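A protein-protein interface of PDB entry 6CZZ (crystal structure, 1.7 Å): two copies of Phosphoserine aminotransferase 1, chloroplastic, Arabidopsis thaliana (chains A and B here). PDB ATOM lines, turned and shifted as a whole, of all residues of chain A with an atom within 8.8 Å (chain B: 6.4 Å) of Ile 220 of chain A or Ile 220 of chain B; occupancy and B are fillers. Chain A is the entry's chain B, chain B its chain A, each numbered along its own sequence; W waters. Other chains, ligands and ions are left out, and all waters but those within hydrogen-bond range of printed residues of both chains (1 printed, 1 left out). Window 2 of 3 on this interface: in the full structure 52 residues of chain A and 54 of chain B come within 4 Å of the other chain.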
ATOM      1  N   ALA A  82       5.193   0.291   9.722  1.00  0.00           N
ATOM      2  CA  ALA A  82       4.568   0.714  10.978  1.00  0.00           C
ATOM      3  C   ALA A  82       3.245   1.439  10.734  1.00  0.00           C
ATOM      4  O   ALA A  82       2.269   1.218  11.454  1.00  0.00           O
ATOM      5  CB  ALA A  82       5.510   1.616  11.772  1.00  0.00           C
ATOM      6  N   PRO A  85      -0.391  -0.942  10.116  1.00  0.00           N
ATOM      7  CA  PRO A  85      -1.164  -1.421  11.278  1.00  0.00           C
ATOM      8  C   PRO A  85      -1.562  -0.305  12.223  1.00  0.00           C
ATOM      9  O   PRO A  85      -2.584  -0.411  12.899  1.00  0.00           O
ATOM     10  CB  PRO A  85      -0.211  -2.428  11.964  1.00  0.00           C
ATOM     11  CG  PRO A  85       1.159  -2.085  11.485  1.00  0.00           C
ATOM     12  CD  PRO A  85       0.920  -1.604  10.042  1.00  0.00           C
ATOM     13  N   LEU A  86      -0.764   0.766  12.345  1.00  0.00           N
ATOM     14  CA  LEU A  86      -1.133   1.822  13.267  1.00  0.00           C
ATOM     15  C   LEU A  86      -2.390   2.522  12.783  1.00  0.00           C
ATOM     16  O   LEU A  86      -3.259   2.883  13.589  1.00  0.00           O
ATOM     17  CB  LEU A  86      -0.008   2.842  13.411  1.00  0.00           C
ATOM     18  CG  LEU A  86       1.204   2.541  14.317  1.00  0.00           C
ATOM     19  CD1 LEU A  86       2.382   3.501  14.142  1.00  0.00           C
ATOM     20  CD2 LEU A  86       0.734   2.537  15.769  1.00  0.00           C
ATOM     21  N   ASN A  87      -2.499   2.715  11.467  1.00  0.00           N
ATOM     22  CA  ASN A  87      -3.687   3.368  10.917  1.00  0.00           C
ATOM     23  C   ASN A  87      -4.878   2.436  10.803  1.00  0.00           C
ATOM     24  O   ASN A  87      -6.021   2.850  11.038  1.00  0.00           O
ATOM     25  CB  ASN A  87      -3.352   3.947   9.547  1.00  0.00           C
ATOM     26  CG  ASN A  87      -2.687   5.274   9.663  1.00  0.00           C
ATOM     27  OD1 ASN A  87      -3.369   6.297   9.738  1.00  0.00           O
ATOM     28  ND2 ASN A  87      -1.360   5.280   9.694  1.00  0.00           N
ATOM     29  N   CYS A  89      -5.544  -0.739  12.041  1.00  0.00           N
ATOM     30  CA  CYS A  89      -5.907  -1.726  13.059  1.00  0.00           C
ATOM     31  C   CYS A  89      -6.001  -1.117  14.441  1.00  0.00           C
ATOM     32  O   CYS A  89      -5.319  -0.135  14.758  1.00  0.00           O
ATOM     33  CB  CYS A  89      -4.869  -2.829  13.139  1.00  0.00           C
ATOM     34  SG  CYS A  89      -4.625  -3.743  11.645  1.00  0.00           S
ATOM     35  N   LYS A  90      -6.847  -1.732  15.275  1.00  0.00           N
ATOM     36  CA  LYS A  90      -6.725  -1.588  16.717  1.00  0.00           C
ATOM     37  C   LYS A  90      -5.631  -2.531  17.208  1.00  0.00           C
ATOM     38  O   LYS A  90      -5.178  -3.436  16.486  1.00  0.00           O
ATOM     39  CB  LYS A  90      -8.069  -1.876  17.390  1.00  0.00           C
ATOM     40  CG  LYS A  90      -9.045  -0.755  17.138  1.00  0.00           C
ATOM     41  CD  LYS A  90     -10.313  -0.897  17.951  1.00  0.00           C
ATOM     42  CE  LYS A  90     -11.258  -1.866  17.329  1.00  0.00           C
ATOM     43  NZ  LYS A  90     -12.631  -1.642  17.876  1.00  0.00           N
ATOM     44  N   SER A  91      -5.201  -2.324  18.443  1.00  0.00           N
ATOM     45  CA  SER A  91      -4.055  -3.093  18.912  1.00  0.00           C
ATOM     46  C   SER A  91      -4.351  -4.575  19.037  1.00  0.00           C
ATOM     47  O   SER A  91      -3.402  -5.359  19.015  1.00  0.00           O
ATOM     48  CB  SER A  91      -3.559  -2.558  20.236  1.00  0.00           C
ATOM     49  OG  SER A  91      -4.559  -2.698  21.218  1.00  0.00           O
ATOM     50  N   GLU A 110       7.708  -5.718  11.934  1.00  0.00           N
ATOM     51  CA  GLU A 110       7.346  -4.384  12.407  1.00  0.00           C
ATOM     52  C   GLU A 110       5.891  -4.336  12.876  1.00  0.00           C
ATOM     53  O   GLU A 110       5.581  -3.684  13.898  1.00  0.00           O
ATOM     54  CB  GLU A 110       7.607  -3.362  11.279  1.00  0.00           C
ATOM     55  CG  GLU A 110       7.360  -1.887  11.650  1.00  0.00           C
ATOM     56  CD  GLU A 110       8.374  -1.331  12.624  1.00  0.00           C
ATOM     57  OE1 GLU A 110       9.129  -2.079  13.245  1.00  0.00           O
ATOM     58  OE2 GLU A 110       8.418  -0.105  12.779  1.00  0.00           O
ATOM     59  N   LYS A 112       4.148  -6.490  14.287  1.00  0.00           N
ATOM     60  CA  LYS A 112       3.968  -7.158  15.580  1.00  0.00           C
ATOM     61  C   LYS A 112       3.973  -6.181  16.743  1.00  0.00           C
ATOM     62  O   LYS A 112       3.422  -6.498  17.800  1.00  0.00           O
ATOM     63  CB  LYS A 112       5.067  -8.211  15.802  1.00  0.00           C
ATOM     64  CG  LYS A 112       4.832  -9.547  15.116  1.00  0.00           C
ATOM     65  CD  LYS A 112       5.955 -10.492  15.540  1.00  0.00           C
ATOM     66  CE  LYS A 112       5.934 -11.797  14.806  1.00  0.00           C
ATOM     67  NZ  LYS A 112       6.902 -12.720  15.499  1.00  0.00           N
ATOM     68  N   LYS A 113       4.611  -5.014  16.576  1.00  0.00           N
ATOM     69  CA  LYS A 113       4.588  -3.975  17.577  1.00  0.00           C
ATOM     70  C   LYS A 113       3.209  -3.400  17.825  1.00  0.00           C
ATOM     71  O   LYS A 113       2.985  -2.860  18.919  1.00  0.00           O
ATOM     72  CB  LYS A 113       5.526  -2.845  17.164  1.00  0.00           C
ATOM     73  CG  LYS A 113       7.002  -3.205  17.179  1.00  0.00           C
ATOM     74  CD  LYS A 113       7.757  -2.053  16.478  1.00  0.00           C
ATOM     75  CE  LYS A 113       9.254  -2.246  16.545  1.00  0.00           C
ATOM     76  NZ  LYS A 113       9.966  -1.138  15.843  1.00  0.00           N
ATOM     77  N   TYR A 114       2.289  -3.531  16.855  1.00  0.00           N
ATOM     78  CA  TYR A 114       1.080  -2.709  16.789  1.00  0.00           C
ATOM     79  C   TYR A 114      -0.207  -3.498  16.715  1.00  0.00           C
ATOM     80  O   TYR A 114      -1.270  -2.914  16.982  1.00  0.00           O
ATOM     81  CB  TYR A 114       1.147  -1.764  15.567  1.00  0.00           C
ATOM     82  CG  TYR A 114       2.413  -0.965  15.622  1.00  0.00           C
ATOM     83  CD1 TYR A 114       2.686  -0.159  16.703  1.00  0.00           C
ATOM     84  CD2 TYR A 114       3.373  -1.059  14.596  1.00  0.00           C
ATOM     85  CE1 TYR A 114       3.905   0.571  16.781  1.00  0.00           C
ATOM     86  CE2 TYR A 114       4.576  -0.311  14.641  1.00  0.00           C
ATOM     87  CZ  TYR A 114       4.830   0.482  15.736  1.00  0.00           C
ATOM     88  OH  TYR A 114       6.008   1.207  15.834  1.00  0.00           O
ATOM     89  N   CYS A 115      -0.158  -4.781  16.391  1.00  0.00           N
ATOM     90  CA  CYS A 115      -1.356  -5.616  16.317  1.00  0.00           C
ATOM     91  C   CYS A 115      -0.915  -7.072  16.313  1.00  0.00           C
ATOM     92  O   CYS A 115       0.270  -7.382  16.444  1.00  0.00           O
ATOM     93  CB  CYS A 115      -2.181  -5.267  15.084  1.00  0.00           C
ATOM     94  SG  CYS A 115      -1.364  -5.655  13.545  1.00  0.00           S
ATOM     95  N   ALA A 217      -6.743   6.114  13.143  1.00  0.00           N
ATOM     96  CA  ALA A 217      -5.456   5.551  13.551  1.00  0.00           C
ATOM     97  C   ALA A 217      -5.411   5.398  15.074  1.00  0.00           C
ATOM     98  O   ALA A 217      -6.169   6.048  15.812  1.00  0.00           O
ATOM     99  CB  ALA A 217      -4.291   6.440  13.098  1.00  0.00           C
ATOM    100  N   GLN A 218      -4.534   4.496  15.539  1.00  0.00           N
ATOM    101  CA  GLN A 218      -4.328   4.290  16.974  1.00  0.00           C
ATOM    102  C   GLN A 218      -3.795   5.567  17.627  1.00  0.00           C
ATOM    103  O   GLN A 218      -3.077   6.344  17.001  1.00  0.00           O
ATOM    104  CB  GLN A 218      -3.326   3.156  17.219  1.00  0.00           C
ATOM    105  CG  GLN A 218      -3.757   1.767  16.731  1.00  0.00           C
ATOM    106  CD  GLN A 218      -2.788   0.645  17.144  1.00  0.00           C
ATOM    107  OE1 GLN A 218      -2.218   0.667  18.225  1.00  0.00           O
ATOM    108  NE2 GLN A 218      -2.610  -0.337  16.272  1.00  0.00           N
ATOM    109  N   ASP A 219      -4.118   5.732  18.925  1.00  0.00           N
ATOM    110  CA  ASP A 219      -3.756   6.919  19.699  1.00  0.00           C
ATOM    111  C   ASP A 219      -2.257   7.208  19.653  1.00  0.00           C
ATOM    112  O   ASP A 219      -1.821   8.371  19.673  1.00  0.00           O
ATOM    113  CB  ASP A 219      -4.208   6.722  21.156  1.00  0.00           C
ATOM    114  CG  ASP A 219      -3.476   5.563  21.865  1.00  0.00           C
ATOM    115  OD1 ASP A 219      -3.263   4.465  21.275  1.00  0.00           O
ATOM    116  OD2 ASP A 219      -3.110   5.750  23.042  1.00  0.00           O
ATOM    117  N   ILE A 220      -1.441   6.148  19.627  1.00  0.00           N
ATOM    118  CA  ILE A 220       0.013   6.314  19.651  1.00  0.00           C
ATOM    119  C   ILE A 220       0.630   6.597  18.286  1.00  0.00           C
ATOM    120  O   ILE A 220       1.856   6.732  18.205  1.00  0.00           O
ATOM    121  CB  ILE A 220       0.708   5.064  20.212  1.00  0.00           C
ATOM    122  CG1 ILE A 220       0.132   3.825  19.501  1.00  0.00           C
ATOM    123  CG2 ILE A 220       0.538   5.016  21.719  1.00  0.00           C
ATOM    124  CD1 ILE A 220       1.014   2.606  19.546  1.00  0.00           C
ATOM    125  N   THR A 221      -0.157   6.677  17.231  1.00  0.00           N
ATOM    126  CA  THR A 221       0.374   6.921  15.892  1.00  0.00           C
ATOM    127  C   THR A 221       1.024   8.299  15.869  1.00  0.00           C
ATOM    128  O   THR A 221       0.353   9.288  16.226  1.00  0.00           O
ATOM    129  CB  THR A 221      -0.754   6.863  14.863  1.00  0.00           C
ATOM    130  OG1 THR A 221      -1.393   5.579  14.949  1.00  0.00           O
ATOM    131  CG2 THR A 221      -0.162   7.065  13.450  1.00  0.00           C
ATOM    132  N   PRO A 222       2.317   8.422  15.538  1.00  0.00           N
ATOM    133  CA  PRO A 222       2.873   9.766  15.346  1.00  0.00           C
ATOM    134  C   PRO A 222       2.074  10.520  14.295  1.00  0.00           C
ATOM    135  O   PRO A 222       1.575   9.939  13.328  1.00  0.00           O
ATOM    136  CB  PRO A 222       4.320   9.514  14.854  1.00  0.00           C
ATOM    137  CG  PRO A 222       4.642   8.112  15.336  1.00  0.00           C
ATOM    138  CD  PRO A 222       3.314   7.352  15.275  1.00  0.00           C
ATOM    139  N   VAL A 223       1.976  11.838  14.479  1.00  0.00           N
ATOM    140  CA  VAL A 223       1.218  12.613  13.510  1.00  0.00           C
ATOM    141  C   VAL A 223       1.775  12.415  12.105  1.00  0.00           C
ATOM    142  O   VAL A 223       1.005  12.303  11.137  1.00  0.00           O
ATOM    143  CB  VAL A 223       1.166  14.090  13.944  1.00  0.00           C
ATOM    144  CG1 VAL A 223       2.517  14.756  13.864  1.00  0.00           C
ATOM    145  CG2 VAL A 223       0.113  14.866  13.132  1.00  0.00           C
ATOM    146  N   MET A 224       3.092  12.242  11.976  1.00  0.00           N
ATOM    147  CA  MET A 224       3.674  12.068  10.656  1.00  0.00           C
ATOM    148  C   MET A 224       3.404  10.709  10.034  1.00  0.00           C
ATOM    149  O   MET A 224       3.775  10.504   8.867  1.00  0.00           O
ATOM    150  CB  MET A 224       5.183  12.295  10.694  1.00  0.00           C
ATOM    151  CG  MET A 224       5.476  13.804  10.940  1.00  0.00           C
ATOM    152  SD  MET A 224       4.848  14.740   9.540  1.00  0.00           S
ATOM    153  CE  MET A 224       5.610  13.879   8.136  1.00  0.00           C
ATOM    154  N   LEU A 225       2.800   9.782  10.751  1.00  0.00           N
ATOM    155  CA  LEU A 225       2.414   8.504  10.150  1.00  0.00           C
ATOM    156  C   LEU A 225       0.898   8.383   9.954  1.00  0.00           C
ATOM    157  O   LEU A 225       0.419   7.345   9.485  1.00  0.00           O
ATOM    158  CB  LEU A 225       2.938   7.326  11.006  1.00  0.00           C
ATOM    159  CG  LEU A 225       4.355   6.805  10.717  1.00  0.00           C
ATOM    160  CD1 LEU A 225       5.404   7.873  10.975  1.00  0.00           C
ATOM    161  CD2 LEU A 225       4.645   5.610  11.596  1.00  0.00           C
ATOM    162  N   ASP A 226       0.147   9.444  10.209  1.00  0.00           N
ATOM    163  CA  ASP A 226      -1.315   9.366  10.278  1.00  0.00           C
ATOM    164  C   ASP A 226      -1.907   9.649   8.897  1.00  0.00           C
ATOM    165  O   ASP A 226      -1.730  10.743   8.350  1.00  0.00           O
ATOM    166  CB  ASP A 226      -1.809  10.362  11.309  1.00  0.00           C
ATOM    167  CG  ASP A 226      -3.292  10.260  11.575  1.00  0.00           C
ATOM    168  OD1 ASP A 226      -4.077  10.428  10.636  1.00  0.00           O
ATOM    169  OD2 ASP A 226      -3.669  10.042  12.749  1.00  0.00           O
ATOM    170  N   LEU B  86       9.928   9.114  22.304  1.00  0.00           N
ATOM    171  CA  LEU B  86       9.907   7.670  22.135  1.00  0.00           C
ATOM    172  C   LEU B  86      11.271   7.069  22.440  1.00  0.00           C
ATOM    173  O   LEU B  86      11.363   5.991  23.028  1.00  0.00           O
ATOM    174  CB  LEU B  86       9.471   7.299  20.725  1.00  0.00           C
ATOM    175  CG  LEU B  86       7.960   7.350  20.456  1.00  0.00           C
ATOM    176  CD1 LEU B  86       7.693   7.306  18.930  1.00  0.00           C
ATOM    177  CD2 LEU B  86       7.240   6.145  21.091  1.00  0.00           C
ATOM    178  N   LYS B 113       1.701  12.252  23.602  1.00  0.00           N
ATOM    179  CA  LYS B 113       1.291  10.903  23.232  1.00  0.00           C
ATOM    180  C   LYS B 113       2.169   9.860  23.886  1.00  0.00           C
ATOM    181  O   LYS B 113       1.736   8.707  24.021  1.00  0.00           O
ATOM    182  CB  LYS B 113       1.371  10.664  21.714  1.00  0.00           C
ATOM    183  CG  LYS B 113       0.358  11.384  20.847  1.00  0.00           C
ATOM    184  CD  LYS B 113       0.719  11.196  19.330  1.00  0.00           C
ATOM    185  CE  LYS B 113      -0.250  11.950  18.481  1.00  0.00           C
ATOM    186  NZ  LYS B 113       0.171  11.910  17.058  1.00  0.00           N
ATOM    187  N   TYR B 114       3.406  10.224  24.238  1.00  0.00           N
ATOM    188  CA  TYR B 114       4.426   9.243  24.558  1.00  0.00           C
ATOM    189  C   TYR B 114       5.001   9.340  25.964  1.00  0.00           C
ATOM    190  O   TYR B 114       5.657   8.385  26.392  1.00  0.00           O
ATOM    191  CB  TYR B 114       5.573   9.323  23.538  1.00  0.00           C
ATOM    192  CG  TYR B 114       5.016   9.200  22.120  1.00  0.00           C
ATOM    193  CD1 TYR B 114       4.369   8.022  21.695  1.00  0.00           C
ATOM    194  CD2 TYR B 114       5.125  10.265  21.217  1.00  0.00           C
ATOM    195  CE1 TYR B 114       3.822   7.921  20.405  1.00  0.00           C
ATOM    196  CE2 TYR B 114       4.599  10.171  19.941  1.00  0.00           C
ATOM    197  CZ  TYR B 114       3.940   8.984  19.551  1.00  0.00           C
ATOM    198  OH  TYR B 114       3.419   8.876  18.279  1.00  0.00           O
ATOM    199  N   ALA B 217      14.943   2.773  23.237  1.00  0.00           N
ATOM    200  CA  ALA B 217      13.668   3.381  22.872  1.00  0.00           C
ATOM    201  C   ALA B 217      12.499   2.539  23.400  1.00  0.00           C
ATOM    202  O   ALA B 217      12.645   1.365  23.739  1.00  0.00           O
ATOM    203  CB  ALA B 217      13.568   3.524  21.353  1.00  0.00           C
ATOM    204  N   GLN B 218      11.318   3.172  23.480  1.00  0.00           N
ATOM    205  CA  GLN B 218      10.095   2.488  23.863  1.00  0.00           C
ATOM    206  C   GLN B 218       9.747   1.383  22.863  1.00  0.00           C
ATOM    207  O   GLN B 218      10.051   1.476  21.670  1.00  0.00           O
ATOM    208  CB  GLN B 218       8.931   3.491  23.961  1.00  0.00           C
ATOM    209  CG  GLN B 218       9.131   4.597  24.978  1.00  0.00           C
ATOM    210  CD  GLN B 218       7.863   5.394  25.194  1.00  0.00           C
ATOM    211  OE1 GLN B 218       6.747   4.840  25.161  1.00  0.00           O
ATOM    212  NE2 GLN B 218       8.012   6.694  25.400  1.00  0.00           N
ATOM    213  N   ASP B 219       9.087   0.334  23.368  1.00  0.00           N
ATOM    214  CA  ASP B 219       8.833  -0.806  22.498  1.00  0.00           C
ATOM    215  C   ASP B 219       7.939  -0.435  21.320  1.00  0.00           C
ATOM    216  O   ASP B 219       8.085  -1.045  20.253  1.00  0.00           O
ATOM    217  CB  ASP B 219       8.238  -1.976  23.278  1.00  0.00           C
ATOM    218  CG  ASP B 219       9.251  -2.658  24.199  1.00  0.00           C
ATOM    219  OD1 ASP B 219      10.488  -2.494  24.022  1.00  0.00           O
ATOM    220  OD2 ASP B 219       8.797  -3.373  25.116  1.00  0.00           O
ATOM    221  N   ILE B 220       7.073   0.578  21.455  1.00  0.00           N
ATOM    222  CA  ILE B 220       6.203   1.012  20.363  1.00  0.00           C
ATOM    223  C   ILE B 220       6.917   1.880  19.336  1.00  0.00           C
ATOM    224  O   ILE B 220       6.278   2.296  18.363  1.00  0.00           O
ATOM    225  CB  ILE B 220       4.969   1.818  20.840  1.00  0.00           C
ATOM    226  CG1 ILE B 220       5.392   2.906  21.853  1.00  0.00           C
ATOM    227  CG2 ILE B 220       3.910   0.892  21.386  1.00  0.00           C
ATOM    228  CD1 ILE B 220       4.343   4.021  22.101  1.00  0.00           C
ATOM    229  N   THR B 221       8.207   2.191  19.529  1.00  0.00           N
ATOM    230  CA  THR B 221       8.932   3.047  18.577  1.00  0.00           C
ATOM    231  C   THR B 221       9.027   2.366  17.198  1.00  0.00           C
ATOM    232  O   THR B 221       9.594   1.273  17.097  1.00  0.00           O
ATOM    233  CB  THR B 221      10.338   3.374  19.113  1.00  0.00           C
ATOM    234  OG1 THR B 221      10.251   3.988  20.417  1.00  0.00           O
ATOM    235  CG2 THR B 221      11.075   4.350  18.143  1.00  0.00           C
ATOM    236  N   PRO B 222       8.481   2.957  16.135  1.00  0.00           N
ATOM    237  CA  PRO B 222       8.737   2.434  14.788  1.00  0.00           C
ATOM    238  C   PRO B 222      10.227   2.298  14.538  1.00  0.00           C
ATOM    239  O   PRO B 222      11.021   3.145  14.956  1.00  0.00           O
ATOM    240  CB  PRO B 222       8.106   3.503  13.874  1.00  0.00           C
ATOM    241  CG  PRO B 222       7.056   4.180  14.760  1.00  0.00           C
ATOM    242  CD  PRO B 222       7.718   4.218  16.119  1.00  0.00           C
ATOM    243  N   VAL B 223      10.625   1.214  13.853  1.00  0.00           N
ATOM    244  CA  VAL B 223      12.057   1.032  13.623  1.00  0.00           C
ATOM    245  C   VAL B 223      12.624   2.256  12.915  1.00  0.00           C
ATOM    246  O   VAL B 223      13.763   2.684  13.197  1.00  0.00           O
ATOM    247  CB  VAL B 223      12.308  -0.284  12.848  1.00  0.00           C
ATOM    248  CG1 VAL B 223      11.845  -0.180  11.363  1.00  0.00           C
ATOM    249  CG2 VAL B 223      13.777  -0.655  12.938  1.00  0.00           C
HETATM  250  O   HOH W   1      -1.059   8.206  23.203  1.00  0.00           O
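The backbone carbonyl oxygen of Thr 221 of chain A is in hydrogen-bond range of the side-chain amino group of Lys 113 of chain B (2.8 Å).
O of Ile 220 of chain A lies within hydrogen-bond range of OH of Tyr 114 of chain B, 2.7 Å away.
O of Ile 220 of chain B lies within hydrogen-bond range of OH of Tyr 114 of chain A.
The side-chain amino group (NZ) of Lys 113 of chain A sits at hydrogen-bond distance from the backbone carbonyl oxygen (O) of Thr 221 of chain B.
The backbone NH (N) of Val 223 of chain B is in hydrogen-bond range of the side-chain carboxylate (OE2) of Glu 110 of chain A, at 2.8 Å.
The side-chain amino group (NZ) of Lys 113 of chain A sits close to the backbone NH (N) of Val 223 of chain B (3.2 Å).
The backbone nitrogen (N) of Pro 222 of chain B lies close to the side-chain hydroxyl (OH) of Tyr 114 of chain A, at 3.0 Å.
N of Pro 222 of chain A lies close to OH of Tyr 114 of chain B, at 3.0 Å.
The backbone NH of Val 223 of chain A sits close to the side-chain amino group of Lys 113 of chain B.
The side-chain hydroxyl of Thr 221 of chain B lies close to the backbone carbonyl oxygen of Leu 86 of chain B, at 3.5 Å.
The backbone carbonyl oxygen of Tyr 114 of chain B lies within hydrogen-bond range of the side-chain amide nitrogen of Gln 218 of chain B (3.1 Å).
The backbone carbonyl oxygen (O) of Gln 218 of chain B sits at hydrogen-bond distance from the side-chain hydroxyl (OG1) of Thr 221 of chain B (2.8 Å).
The side-chain carboxylate (OE1) of Glu 110 of chain A lies within salt-bridge range of the side-chain amino group (NZ) of Lys 113 of chain A, at 2.9 Å.
The backbone carbonyl oxygen of Tyr 114 of chain A lies within hydrogen-bond range of the side-chain amide nitrogen of Gln 218 of chain A.
The side-chain hydroxyl of Thr 221 of chain A lies within hydrogen-bond range of the backbone carbonyl oxygen of Gln 218 of chain A (2.8 Å).
CB of Ala 82 of chain A touches CB of Pro 222 of chain B, 3.8 Å away.
CA of Pro 222 of chain B touches OE2 of Glu 110 of chain A, at 3.3 Å.
Asp 219 of chain B touches Lys 113 of chain A.
NZ of Lys 113 of chain A touches C of Pro 222 of chain B, 3.7 Å away.
Thr 221 of chain B touches Tyr 114 of chain A (C to OH, 3.5 Å).
CD of Lys 113 of chain B touches O of Asp 219 of chain A (3.8 Å).
Ile 220 of chain B touches Ile 220 of chain A.
Thr 221 of chain A touches Tyr 114 of chain B (C to OH, 3.4 Å).
Pro 222 of chain A touches Lys 113 of chain B.
Of the printed residues of chain B, Glu 110 of chain A touches Pro 222 and Val 223.
Ile 220 of chain A touches two residues of chain B.
Ala 217 of chain B touches none of the printed residues of chain A.
Ile 220 of chain B touches just these residues of chain A: Tyr 114 and Ile 220.
Printed residues of chain A within 4 Å of Pro 222 of chain B: Ala 82 (3.8 Å), Glu 110 (3.3 Å), Lys 113 (3.7 Å) and Tyr 114 (3.0 Å).
The nearest residue of chain B that does not touch Ile 220 of chain A is Lys 113 of chain B (4.5 Å).
The nearest residue of chain A that does not touch Ile 220 of chain B is Lys 113 of chain A (4.6 Å).
The nearest printed residue of chain B that does not touch Pro 222 of chain A is Pro 222 of chain B (4.6 Å).
Printed residues of chain B that touch a printed residue of chain A: Lys 113, Tyr 114, Asp 219, Ile 220, Thr 221, Pro 222 and Val 223.
Along chain B the printed residues that touch a printed residue of chain A span positions 113 to 223.
Printed residues of chain A that touch a printed residue of chain B: Ala 82, Glu 110, Lys 113, Tyr 114, Asp 219, Ile 220, Thr 221, Pro 222 and Val 223.
Hydrophobic or aromatic side chains of chain A that line the printed part of chain B: Ala 82, Tyr 114, Ile 220, Pro 222 and Val 223.
Among the printed residues, 18 pairs touch across the chains.
Among the printed residues, no Asp or Glu carboxylate lies within 4 Å of a Lys or Arg side-chain nitrogen of the other chain.
Lys 113 of chain A touches Asp 219 of chain B, and with the chains exchanged Asp 219 of chain A touches Lys 113 of chain B.
Tyr 114 of chain A touches Thr 221 of chain B, and with the chains exchanged Thr 221 of chain A touches Tyr 114 of chain B.
Tyr 114 of chain A touches Pro 222 of chain B, and with the chains exchanged Pro 222 of chain A touches Tyr 114 of chain B.
Ile 220 of chain A touches its own counterpart, Ile 220 of chain B.
Water W1 bridges O of Lys 113 of chain B (3.0 Å) and OD2 of Asp 219 of chain A (3.2 Å).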
